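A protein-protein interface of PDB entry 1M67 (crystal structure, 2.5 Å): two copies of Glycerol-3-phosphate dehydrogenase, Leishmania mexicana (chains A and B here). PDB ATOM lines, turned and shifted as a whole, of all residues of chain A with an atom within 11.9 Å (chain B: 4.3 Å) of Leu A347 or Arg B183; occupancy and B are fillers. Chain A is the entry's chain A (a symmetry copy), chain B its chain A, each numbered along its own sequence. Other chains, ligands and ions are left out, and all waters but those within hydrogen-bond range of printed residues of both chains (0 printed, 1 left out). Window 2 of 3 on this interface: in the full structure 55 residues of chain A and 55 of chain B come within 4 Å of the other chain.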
ATOM      1  N   ARG A 236      -6.019  -9.685 -17.806  1.00  0.00           N
ATOM      2  CA  ARG A 236      -5.358  -9.093 -16.633  1.00  0.00           C
ATOM      3  C   ARG A 236      -6.364  -8.316 -15.786  1.00  0.00           C
ATOM      4  O   ARG A 236      -6.329  -8.362 -14.562  1.00  0.00           O
ATOM      5  CB  ARG A 236      -4.192  -8.178 -17.036  1.00  0.00           C
ATOM      6  CG  ARG A 236      -3.162  -8.838 -17.960  1.00  0.00           C
ATOM      7  CD  ARG A 236      -2.483 -10.057 -17.356  1.00  0.00           C
ATOM      8  NE  ARG A 236      -1.905  -9.721 -16.057  1.00  0.00           N
ATOM      9  CZ  ARG A 236      -1.252 -10.569 -15.282  1.00  0.00           C
ATOM     10  NH1 ARG A 236      -1.086 -11.828 -15.656  1.00  0.00           N
ATOM     11  NH2 ARG A 236      -0.768 -10.158 -14.124  1.00  0.00           N
ATOM     12  N   ALA A 340       3.395   2.623 -20.457  1.00  0.00           N
ATOM     13  CA  ALA A 340       4.790   2.306 -20.130  1.00  0.00           C
ATOM     14  C   ALA A 340       4.996   2.003 -18.660  1.00  0.00           C
ATOM     15  O   ALA A 340       5.752   1.103 -18.316  1.00  0.00           O
ATOM     16  CB  ALA A 340       5.737   3.442 -20.570  1.00  0.00           C
ATOM     17  N   ASP A 341       4.343   2.768 -17.792  1.00  0.00           N
ATOM     18  CA  ASP A 341       4.480   2.546 -16.355  1.00  0.00           C
ATOM     19  C   ASP A 341       3.888   1.204 -15.972  1.00  0.00           C
ATOM     20  O   ASP A 341       4.430   0.476 -15.146  1.00  0.00           O
ATOM     21  CB  ASP A 341       3.799   3.660 -15.568  1.00  0.00           C
ATOM     22  CG  ASP A 341       4.712   4.832 -15.339  1.00  0.00           C
ATOM     23  OD1 ASP A 341       4.227   5.927 -14.973  1.00  0.00           O
ATOM     24  OD2 ASP A 341       5.945   4.731 -15.505  1.00  0.00           O
ATOM     25  N   LEU A 342       2.764   0.892 -16.602  1.00  0.00           N
ATOM     26  CA  LEU A 342       2.079  -0.357 -16.394  1.00  0.00           C
ATOM     27  C   LEU A 342       3.019  -1.486 -16.794  1.00  0.00           C
ATOM     28  O   LEU A 342       3.053  -2.541 -16.148  1.00  0.00           O
ATOM     29  CB  LEU A 342       0.849  -0.380 -17.281  1.00  0.00           C
ATOM     30  CG  LEU A 342      -0.491  -0.855 -16.757  1.00  0.00           C
ATOM     31  CD1 LEU A 342      -1.224  -1.448 -17.944  1.00  0.00           C
ATOM     32  CD2 LEU A 342      -0.323  -1.861 -15.612  1.00  0.00           C
ATOM     33  N   LEU A 343       3.790  -1.254 -17.861  1.00  0.00           N
ATOM     34  CA  LEU A 343       4.753  -2.244 -18.344  1.00  0.00           C
ATOM     35  C   LEU A 343       6.135  -2.104 -17.689  1.00  0.00           C
ATOM     36  O   LEU A 343       7.062  -2.827 -18.045  1.00  0.00           O
ATOM     37  CB  LEU A 343       4.893  -2.190 -19.874  1.00  0.00           C
ATOM     38  CG  LEU A 343       3.640  -2.307 -20.753  1.00  0.00           C
ATOM     39  CD1 LEU A 343       3.998  -2.222 -22.221  1.00  0.00           C
ATOM     40  CD2 LEU A 343       2.877  -3.588 -20.474  1.00  0.00           C
ATOM     41  N   SER A 344       6.270  -1.186 -16.735  1.00  0.00           N
ATOM     42  CA  SER A 344       7.542  -0.992 -16.033  1.00  0.00           C
ATOM     43  C   SER A 344       7.889  -2.156 -15.106  1.00  0.00           C
ATOM     44  O   SER A 344       9.016  -2.268 -14.622  1.00  0.00           O
ATOM     45  CB  SER A 344       7.511   0.300 -15.212  1.00  0.00           C
ATOM     46  OG  SER A 344       6.675   0.160 -14.067  1.00  0.00           O
ATOM     47  N   CYS A 345       6.916  -3.027 -14.876  1.00  0.00           N
ATOM     48  CA  CYS A 345       7.073  -4.156 -13.959  1.00  0.00           C
ATOM     49  C   CYS A 345       8.191  -5.128 -14.318  1.00  0.00           C
ATOM     50  O   CYS A 345       8.787  -5.741 -13.439  1.00  0.00           O
ATOM     51  CB  CYS A 345       5.755  -4.927 -13.862  1.00  0.00           C
ATOM     52  SG  CYS A 345       5.100  -5.452 -15.479  1.00  0.00           S
ATOM     53  N   GLY A 346       8.464  -5.283 -15.606  1.00  0.00           N
ATOM     54  CA  GLY A 346       9.454  -6.251 -16.036  1.00  0.00           C
ATOM     55  C   GLY A 346       8.834  -7.618 -16.288  1.00  0.00           C
ATOM     56  O   GLY A 346       7.631  -7.823 -16.106  1.00  0.00           O
ATOM     57  N   LEU A 347       9.669  -8.565 -16.697  1.00  0.00           N
ATOM     58  CA  LEU A 347       9.212  -9.905 -17.033  1.00  0.00           C
ATOM     59  C   LEU A 347       8.633 -10.682 -15.842  1.00  0.00           C
ATOM     60  O   LEU A 347       9.316 -10.919 -14.843  1.00  0.00           O
ATOM     61  CB  LEU A 347      10.339 -10.664 -17.729  1.00  0.00           C
ATOM     62  CG  LEU A 347      10.684  -9.950 -19.042  1.00  0.00           C
ATOM     63  CD1 LEU A 347      11.762 -10.667 -19.825  1.00  0.00           C
ATOM     64  CD2 LEU A 347       9.433  -9.789 -19.894  1.00  0.00           C
ATOM     65  N   GLN A 348       7.364 -11.071 -15.958  1.00  0.00           N
ATOM     66  CA  GLN A 348       6.670 -11.758 -14.866  1.00  0.00           C
ATOM     67  C   GLN A 348       6.068 -13.120 -15.216  1.00  0.00           C
ATOM     68  O   GLN A 348       5.951 -13.488 -16.380  1.00  0.00           O
ATOM     69  CB  GLN A 348       5.559 -10.870 -14.317  1.00  0.00           C
ATOM     70  CG  GLN A 348       6.034  -9.699 -13.472  1.00  0.00           C
ATOM     71  CD  GLN A 348       4.879  -8.799 -13.051  1.00  0.00           C
ATOM     72  OE1 GLN A 348       3.760  -8.949 -13.549  1.00  0.00           O
ATOM     73  NE2 GLN A 348       5.145  -7.870 -12.130  1.00  0.00           N
ATOM     74  N   ASP A 349       5.703 -13.869 -14.181  1.00  0.00           N
ATOM     75  CA  ASP A 349       4.987 -15.123 -14.343  1.00  0.00           C
ATOM     76  C   ASP A 349       3.537 -14.741 -14.531  1.00  0.00           C
ATOM     77  O   ASP A 349       3.108 -13.682 -14.057  1.00  0.00           O
ATOM     78  CB  ASP A 349       5.080 -15.960 -13.080  1.00  0.00           C
ATOM     79  CG  ASP A 349       6.358 -16.734 -12.986  1.00  0.00           C
ATOM     80  OD1 ASP A 349       7.193 -16.660 -13.918  1.00  0.00           O
ATOM     81  OD2 ASP A 349       6.611 -17.448 -12.000  1.00  0.00           O
ATOM     82  N   GLU A 350       2.768 -15.592 -15.196  1.00  0.00           N
ATOM     83  CA  GLU A 350       1.359 -15.279 -15.375  1.00  0.00           C
ATOM     84  C   GLU A 350       0.638 -15.062 -14.042  1.00  0.00           C
ATOM     85  O   GLU A 350      -0.254 -14.236 -13.955  1.00  0.00           O
ATOM     86  CB  GLU A 350       0.643 -16.312 -16.253  1.00  0.00           C
ATOM     87  CG  GLU A 350      -0.769 -15.894 -16.607  1.00  0.00           C
ATOM     88  CD  GLU A 350      -1.272 -16.488 -17.909  1.00  0.00           C
ATOM     89  OE1 GLU A 350      -1.085 -17.714 -18.134  1.00  0.00           O
ATOM     90  OE2 GLU A 350      -1.876 -15.717 -18.691  1.00  0.00           O
ATOM     91  N   GLY A 351       1.046 -15.774 -12.993  1.00  0.00           N
ATOM     92  CA  GLY A 351       0.454 -15.584 -11.671  1.00  0.00           C
ATOM     93  C   GLY A 351      -0.925 -16.175 -11.364  1.00  0.00           C
ATOM     94  O   GLY A 351      -1.648 -15.690 -10.466  1.00  0.00           O
ATOM     95  N   LYS B   9      14.046 -12.946 -14.449  1.00  0.00           N
ATOM     96  CA  LYS B   9      14.890 -11.757 -14.773  1.00  0.00           C
ATOM     97  C   LYS B   9      14.178 -10.872 -15.796  1.00  0.00           C
ATOM     98  O   LYS B   9      13.574 -11.371 -16.750  1.00  0.00           O
ATOM     99  CB  LYS B   9      16.267 -12.186 -15.294  1.00  0.00           C
ATOM    100  CG  LYS B   9      17.320 -11.082 -15.268  1.00  0.00           C
ATOM    101  N   ASP B  10      14.257  -9.560 -15.589  1.00  0.00           N
ATOM    102  CA  ASP B  10      13.593  -8.594 -16.459  1.00  0.00           C
ATOM    103  C   ASP B  10      14.515  -8.047 -17.571  1.00  0.00           C
ATOM    104  O   ASP B  10      14.225  -7.004 -18.166  1.00  0.00           O
ATOM    105  CB  ASP B  10      13.026  -7.444 -15.613  1.00  0.00           C
ATOM    106  CG  ASP B  10      12.214  -7.936 -14.409  1.00  0.00           C
ATOM    107  OD1 ASP B  10      12.601  -8.956 -13.790  1.00  0.00           O
ATOM    108  OD2 ASP B  10      11.173  -7.360 -14.005  1.00  0.00           O
ATOM    109  N   GLU B  11      15.607  -8.763 -17.851  1.00  0.00           N
ATOM    110  CA  GLU B  11      16.598  -8.354 -18.856  1.00  0.00           C
ATOM    111  C   GLU B  11      16.596  -9.284 -20.079  1.00  0.00           C
ATOM    112  O   GLU B  11      16.713 -10.500 -19.947  1.00  0.00           O
ATOM    113  CB  GLU B  11      17.995  -8.312 -18.223  1.00  0.00           C
ATOM    114  CG  GLU B  11      19.028  -7.488 -18.978  1.00  0.00           C
ATOM    115  CD  GLU B  11      20.402  -7.542 -18.328  1.00  0.00           C
ATOM    116  OE1 GLU B  11      20.723  -6.624 -17.540  1.00  0.00           O
ATOM    117  OE2 GLU B  11      21.157  -8.503 -18.601  1.00  0.00           O
ATOM    118  N   LEU B  12      16.501  -8.706 -21.270  1.00  0.00           N
ATOM    119  CA  LEU B  12      16.330  -9.494 -22.489  1.00  0.00           C
ATOM    120  C   LEU B  12      17.561 -10.220 -23.026  1.00  0.00           C
ATOM    121  O   LEU B  12      18.698  -9.918 -22.668  1.00  0.00           O
ATOM    122  CB  LEU B  12      15.729  -8.623 -23.592  1.00  0.00           C
ATOM    123  CG  LEU B  12      14.459  -7.858 -23.220  1.00  0.00           C
ATOM    124  CD1 LEU B  12      14.000  -7.054 -24.408  1.00  0.00           C
ATOM    125  CD2 LEU B  12      13.363  -8.800 -22.767  1.00  0.00           C
ATOM    126  N   LEU B  13      17.306 -11.179 -23.907  1.00  0.00           N
ATOM    127  CA  LEU B  13      18.364 -11.940 -24.538  1.00  0.00           C
ATOM    128  C   LEU B  13      18.288 -11.782 -26.044  1.00  0.00           C
ATOM    129  O   LEU B  13      17.229 -11.932 -26.636  1.00  0.00           O
ATOM    130  CB  LEU B  13      18.260 -13.427 -24.179  1.00  0.00           C
ATOM    131  CG  LEU B  13      18.594 -13.829 -22.743  1.00  0.00           C
ATOM    132  CD1 LEU B  13      18.393 -15.342 -22.554  1.00  0.00           C
ATOM    133  CD2 LEU B  13      20.011 -13.397 -22.339  1.00  0.00           C
ATOM    134  N   LYS B  37      15.182  -9.595 -32.443  1.00  0.00           N
ATOM    135  CA  LYS B  37      15.919 -10.105 -31.296  1.00  0.00           C
ATOM    136  C   LYS B  37      17.059 -11.008 -31.731  1.00  0.00           C
ATOM    137  O   LYS B  37      17.962 -11.325 -30.936  1.00  0.00           O
ATOM    138  CB  LYS B  37      14.979 -10.838 -30.347  1.00  0.00           C
ATOM    139  CG  LYS B  37      13.886  -9.964 -29.750  1.00  0.00           C
ATOM    140  CD  LYS B  37      14.441  -8.925 -28.792  1.00  0.00           C
ATOM    141  CE  LYS B  37      15.337  -9.537 -27.735  1.00  0.00           C
ATOM    142  NZ  LYS B  37      14.674 -10.679 -26.997  1.00  0.00           N
ATOM    143  N   ARG B 179      10.980 -18.972 -18.541  1.00  0.00           N
ATOM    144  CA  ARG B 179      11.506 -17.655 -18.226  1.00  0.00           C
ATOM    145  C   ARG B 179      12.646 -17.296 -19.149  1.00  0.00           C
ATOM    146  O   ARG B 179      12.825 -16.134 -19.485  1.00  0.00           O
ATOM    147  CB  ARG B 179      11.959 -17.582 -16.769  1.00  0.00           C
ATOM    148  CG  ARG B 179      10.834 -17.705 -15.756  1.00  0.00           C
ATOM    149  CD  ARG B 179      11.314 -17.632 -14.333  1.00  0.00           C
ATOM    150  NE  ARG B 179      10.240 -17.760 -13.352  1.00  0.00           N
ATOM    151  CZ  ARG B 179      10.425 -18.243 -12.127  1.00  0.00           C
ATOM    152  NH1 ARG B 179      11.644 -18.642 -11.775  1.00  0.00           N
ATOM    153  NH2 ARG B 179       9.405 -18.339 -11.269  1.00  0.00           N
ATOM    154  N   ARG B 180      13.414 -18.286 -19.576  1.00  0.00           N
ATOM    155  CA  ARG B 180      14.511 -18.024 -20.504  1.00  0.00           C
ATOM    156  C   ARG B 180      13.977 -17.791 -21.913  1.00  0.00           C
ATOM    157  O   ARG B 180      14.560 -17.037 -22.677  1.00  0.00           O
ATOM    158  CB  ARG B 180      15.520 -19.180 -20.499  1.00  0.00           C
ATOM    159  CG  ARG B 180      16.595 -19.050 -21.567  1.00  0.00           C
ATOM    160  CD  ARG B 180      17.869 -19.842 -21.310  1.00  0.00           C
ATOM    161  NE  ARG B 180      18.907 -19.530 -22.294  1.00  0.00           N
ATOM    162  CZ  ARG B 180      19.946 -18.729 -22.060  1.00  0.00           C
ATOM    163  NH1 ARG B 180      20.101 -18.159 -20.874  1.00  0.00           N
ATOM    164  NH2 ARG B 180      20.835 -18.496 -23.018  1.00  0.00           N
ATOM    165  N   LEU B 181      12.874 -18.447 -22.263  1.00  0.00           N
ATOM    166  CA  LEU B 181      12.262 -18.241 -23.572  1.00  0.00           C
ATOM    167  C   LEU B 181      11.536 -16.898 -23.553  1.00  0.00           C
ATOM    168  O   LEU B 181      11.442 -16.216 -24.557  1.00  0.00           O
ATOM    169  CB  LEU B 181      11.291 -19.375 -23.917  1.00  0.00           C
ATOM    170  CG  LEU B 181      11.872 -20.747 -24.270  1.00  0.00           C
ATOM    171  CD1 LEU B 181      12.194 -20.914 -25.742  1.00  0.00           C
ATOM    172  CD2 LEU B 181      13.084 -21.088 -23.423  1.00  0.00           C
ATOM    173  N   GLN B 182      11.039 -16.544 -22.379  1.00  0.00           N
ATOM    174  CA  GLN B 182      10.352 -15.300 -22.147  1.00  0.00           C
ATOM    175  C   GLN B 182      11.294 -14.127 -22.452  1.00  0.00           C
ATOM    176  O   GLN B 182      10.851 -13.031 -22.812  1.00  0.00           O
ATOM    177  CB  GLN B 182       9.946 -15.256 -20.677  1.00  0.00           C
ATOM    178  CG  GLN B 182       9.006 -14.155 -20.278  1.00  0.00           C
ATOM    179  CD  GLN B 182       8.634 -14.212 -18.795  1.00  0.00           C
ATOM    180  OE1 GLN B 182       9.354 -14.799 -17.983  1.00  0.00           O
ATOM    181  NE2 GLN B 182       7.513 -13.604 -18.445  1.00  0.00           N
ATOM    182  N   ARG B 183      12.597 -14.373 -22.297  1.00  0.00           N
ATOM    183  CA  ARG B 183      13.606 -13.343 -22.455  1.00  0.00           C
ATOM    184  C   ARG B 183      14.152 -13.283 -23.873  1.00  0.00           C
ATOM    185  O   ARG B 183      14.831 -12.320 -24.239  1.00  0.00           O
ATOM    186  CB  ARG B 183      14.729 -13.536 -21.434  1.00  0.00           C
ATOM    187  CG  ARG B 183      14.254 -13.423 -19.978  1.00  0.00           C
ATOM    188  CD  ARG B 183      15.371 -13.239 -18.971  1.00  0.00           C
ATOM    189  NE  ARG B 183      16.617 -13.832 -19.443  1.00  0.00           N
ATOM    190  CZ  ARG B 183      17.799 -13.632 -18.882  1.00  0.00           C
ATOM    191  NH1 ARG B 183      17.911 -12.856 -17.815  1.00  0.00           N
ATOM    192  NH2 ARG B 183      18.875 -14.210 -19.391  1.00  0.00           N
ATOM    193  N   ILE B 184      13.830 -14.284 -24.681  1.00  0.00           N
ATOM    194  CA  ILE B 184      14.273 -14.321 -26.069  1.00  0.00           C
ATOM    195  C   ILE B 184      13.172 -13.835 -27.000  1.00  0.00           C
ATOM    196  O   ILE B 184      13.438 -13.294 -28.072  1.00  0.00           O
ATOM    197  CB  ILE B 184      14.657 -15.762 -26.451  1.00  0.00           C
ATOM    198  CG1 ILE B 184      15.963 -16.178 -25.764  1.00  0.00           C
ATOM    199  CG2 ILE B 184      14.746 -15.939 -27.954  1.00  0.00           C
ATOM    200  CD1 ILE B 184      16.372 -17.638 -26.047  1.00  0.00           C
ATOM    201  N   MET B 185      11.929 -14.005 -26.572  1.00  0.00           N
ATOM    202  CA  MET B 185      10.782 -13.704 -27.426  1.00  0.00           C
ATOM    203  C   MET B 185      10.232 -12.313 -27.164  1.00  0.00           C
ATOM    204  O   MET B 185       9.556 -11.750 -28.002  1.00  0.00           O
ATOM    205  CB  MET B 185       9.657 -14.722 -27.202  1.00  0.00           C
ATOM    206  CG  MET B 185      10.056 -16.146 -27.423  1.00  0.00           C
ATOM    207  SD  MET B 185      10.889 -16.345 -28.995  1.00  0.00           S
ATOM    208  CE  MET B 185       9.535 -16.091 -30.062  1.00  0.00           C
ATOM    209  N   SER B 186      10.504 -11.785 -25.979  1.00  0.00           N
ATOM    210  CA  SER B 186      10.043 -10.460 -25.645  1.00  0.00           C
ATOM    211  C   SER B 186      10.882  -9.389 -26.367  1.00  0.00           C
ATOM    212  O   SER B 186      12.114  -9.413 -26.320  1.00  0.00           O
ATOM    213  CB  SER B 186      10.076 -10.261 -24.141  1.00  0.00           C
ATOM    214  OG  SER B 186       9.014 -10.959 -23.548  1.00  0.00           O
ATOM    215  N   ARG B 190       8.744  -3.435 -25.866  1.00  0.00           N
ATOM    216  CA  ARG B 190       7.601  -3.979 -25.123  1.00  0.00           C
ATOM    217  C   ARG B 190       6.356  -4.092 -25.985  1.00  0.00           C
ATOM    218  O   ARG B 190       5.269  -3.893 -25.490  1.00  0.00           O
ATOM    219  CB  ARG B 190       7.254  -3.201 -23.843  1.00  0.00           C
ATOM    220  CG  ARG B 190       8.412  -2.906 -22.885  1.00  0.00           C
ATOM    221  CD  ARG B 190       8.793  -4.034 -21.927  1.00  0.00           C
ATOM    222  NE  ARG B 190       7.783  -4.319 -20.898  1.00  0.00           N
ATOM    223  CZ  ARG B 190       7.672  -5.496 -20.266  1.00  0.00           C
ATOM    224  NH1 ARG B 190       8.510  -6.479 -20.553  1.00  0.00           N
ATOM    225  NH2 ARG B 190       6.732  -5.689 -19.349  1.00  0.00           N
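OD2 of Asp B10 sits at hydrogen-bond distance from N of Leu A347 (3.3 Å).
NH2 of Arg B179 is in salt-bridge range of OD2 of Asp A349, at 3.0 Å.
The side-chain amide nitrogen (NE2) of Gln B182 is in hydrogen-bond range of the backbone carbonyl oxygen (O) of Gln A348, 2.6 Å away.
NH2 of Arg B190 lies within hydrogen-bond range of O of Leu A343, 3.2 Å away.
O of Cys A345 lies close to OD2 of Asp B10 (2.9 Å).
The guanidinium group (NE) of Arg B183 sits close to the backbone carbonyl oxygen (O) of Glu B11.
N of Leu B13 sits at hydrogen-bond distance from O of Arg B183, 2.7 Å away.
The backbone carbonyl oxygen (O) of Arg B183 is in hydrogen-bond range of the side-chain amino group (NZ) of Lys B37 (3.2 Å).
NZ of Lys B37 lies within hydrogen-bond range of O of Ser B186 (2.9 Å).
OG of Ser B186 lies within hydrogen-bond range of O of Gln B182 (2.9 Å).
The side-chain sulfur (SG) of Cys A345 is in hydrogen-bond range of the backbone carbonyl oxygen (O) of Leu A342, 3.6 Å away.
CA of Gly A346 touches OD2 of Asp B10, 2.9 Å away.
NH2 of Arg B190 touches O of Gly A346, at 3.98 Å.
Leu A347 touches Lys B9 (CB to O, 3.5 Å).
CD1 of Leu A347 touches CD2 of Leu B12 (3.8 Å).
Leu A347 touches Gln B182 (CD1 to O, 3.9 Å).
Arg B183 touches Leu A347 (CG to CD1, 3.7 Å).
OG of Ser B186 touches CD2 of Leu A347, 3.9 Å away.
Leu A347 touches Arg B190 (CD2 to NH1, 3.5 Å).
Ala A340 touches none of the printed residues of chain B.
Printed residues of chain B within 4 Å of Leu A343: Arg B190.
Of chain B, only Lys B9, Asp B10, Leu B12, Gln B182, Arg B183, Ser B186 and Arg B190 come within 4 Å of Leu A347.
No residue of chain A comes within 4 Å of Glu B11.
Leu B12 touches just one residue of chain A: Leu A347 (3.8 Å).
No residue of chain A comes within 4 Å of Leu B13.
Printed residues of chain A within 4 Å of Arg B179: Asp A349 (3.0 Å).
No residue of chain A comes within 4 Å of Arg B180.
Gln B182 touches just these residues of chain A: Leu A347 (3.9 Å) and Gln A348 (2.6 Å).
Arg B183 touches one residue of chain A.
No residue of chain A comes within 4 Å of Ile B184.
Of chain A, only Leu A347 (3.9 Å) comes within 4 Å of Ser B186.
Of the printed residues of chain A, Arg B190 touches Leu A343 (3.2 Å), Gly A346 (3.98 Å) and Leu A347 (3.5 Å).
Of the 13 printed residues of chain A, 6 touch a printed residue of chain B.
Printed residues of chain A that touch a printed residue of chain B: Leu A343, Cys A345, Gly A346, Leu A347, Gln A348 and Asp A349.
Hydrophobic or aromatic side chains of chain A within 4 Å of the printed part of chain B: Leu A343 and Leu A347.
Among the printed residues, Asp or Glu carboxylates within 4 Å of a Lys or Arg side-chain nitrogen of the other chain: Asp A349 with Arg B179.
No position is printed for both chains.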
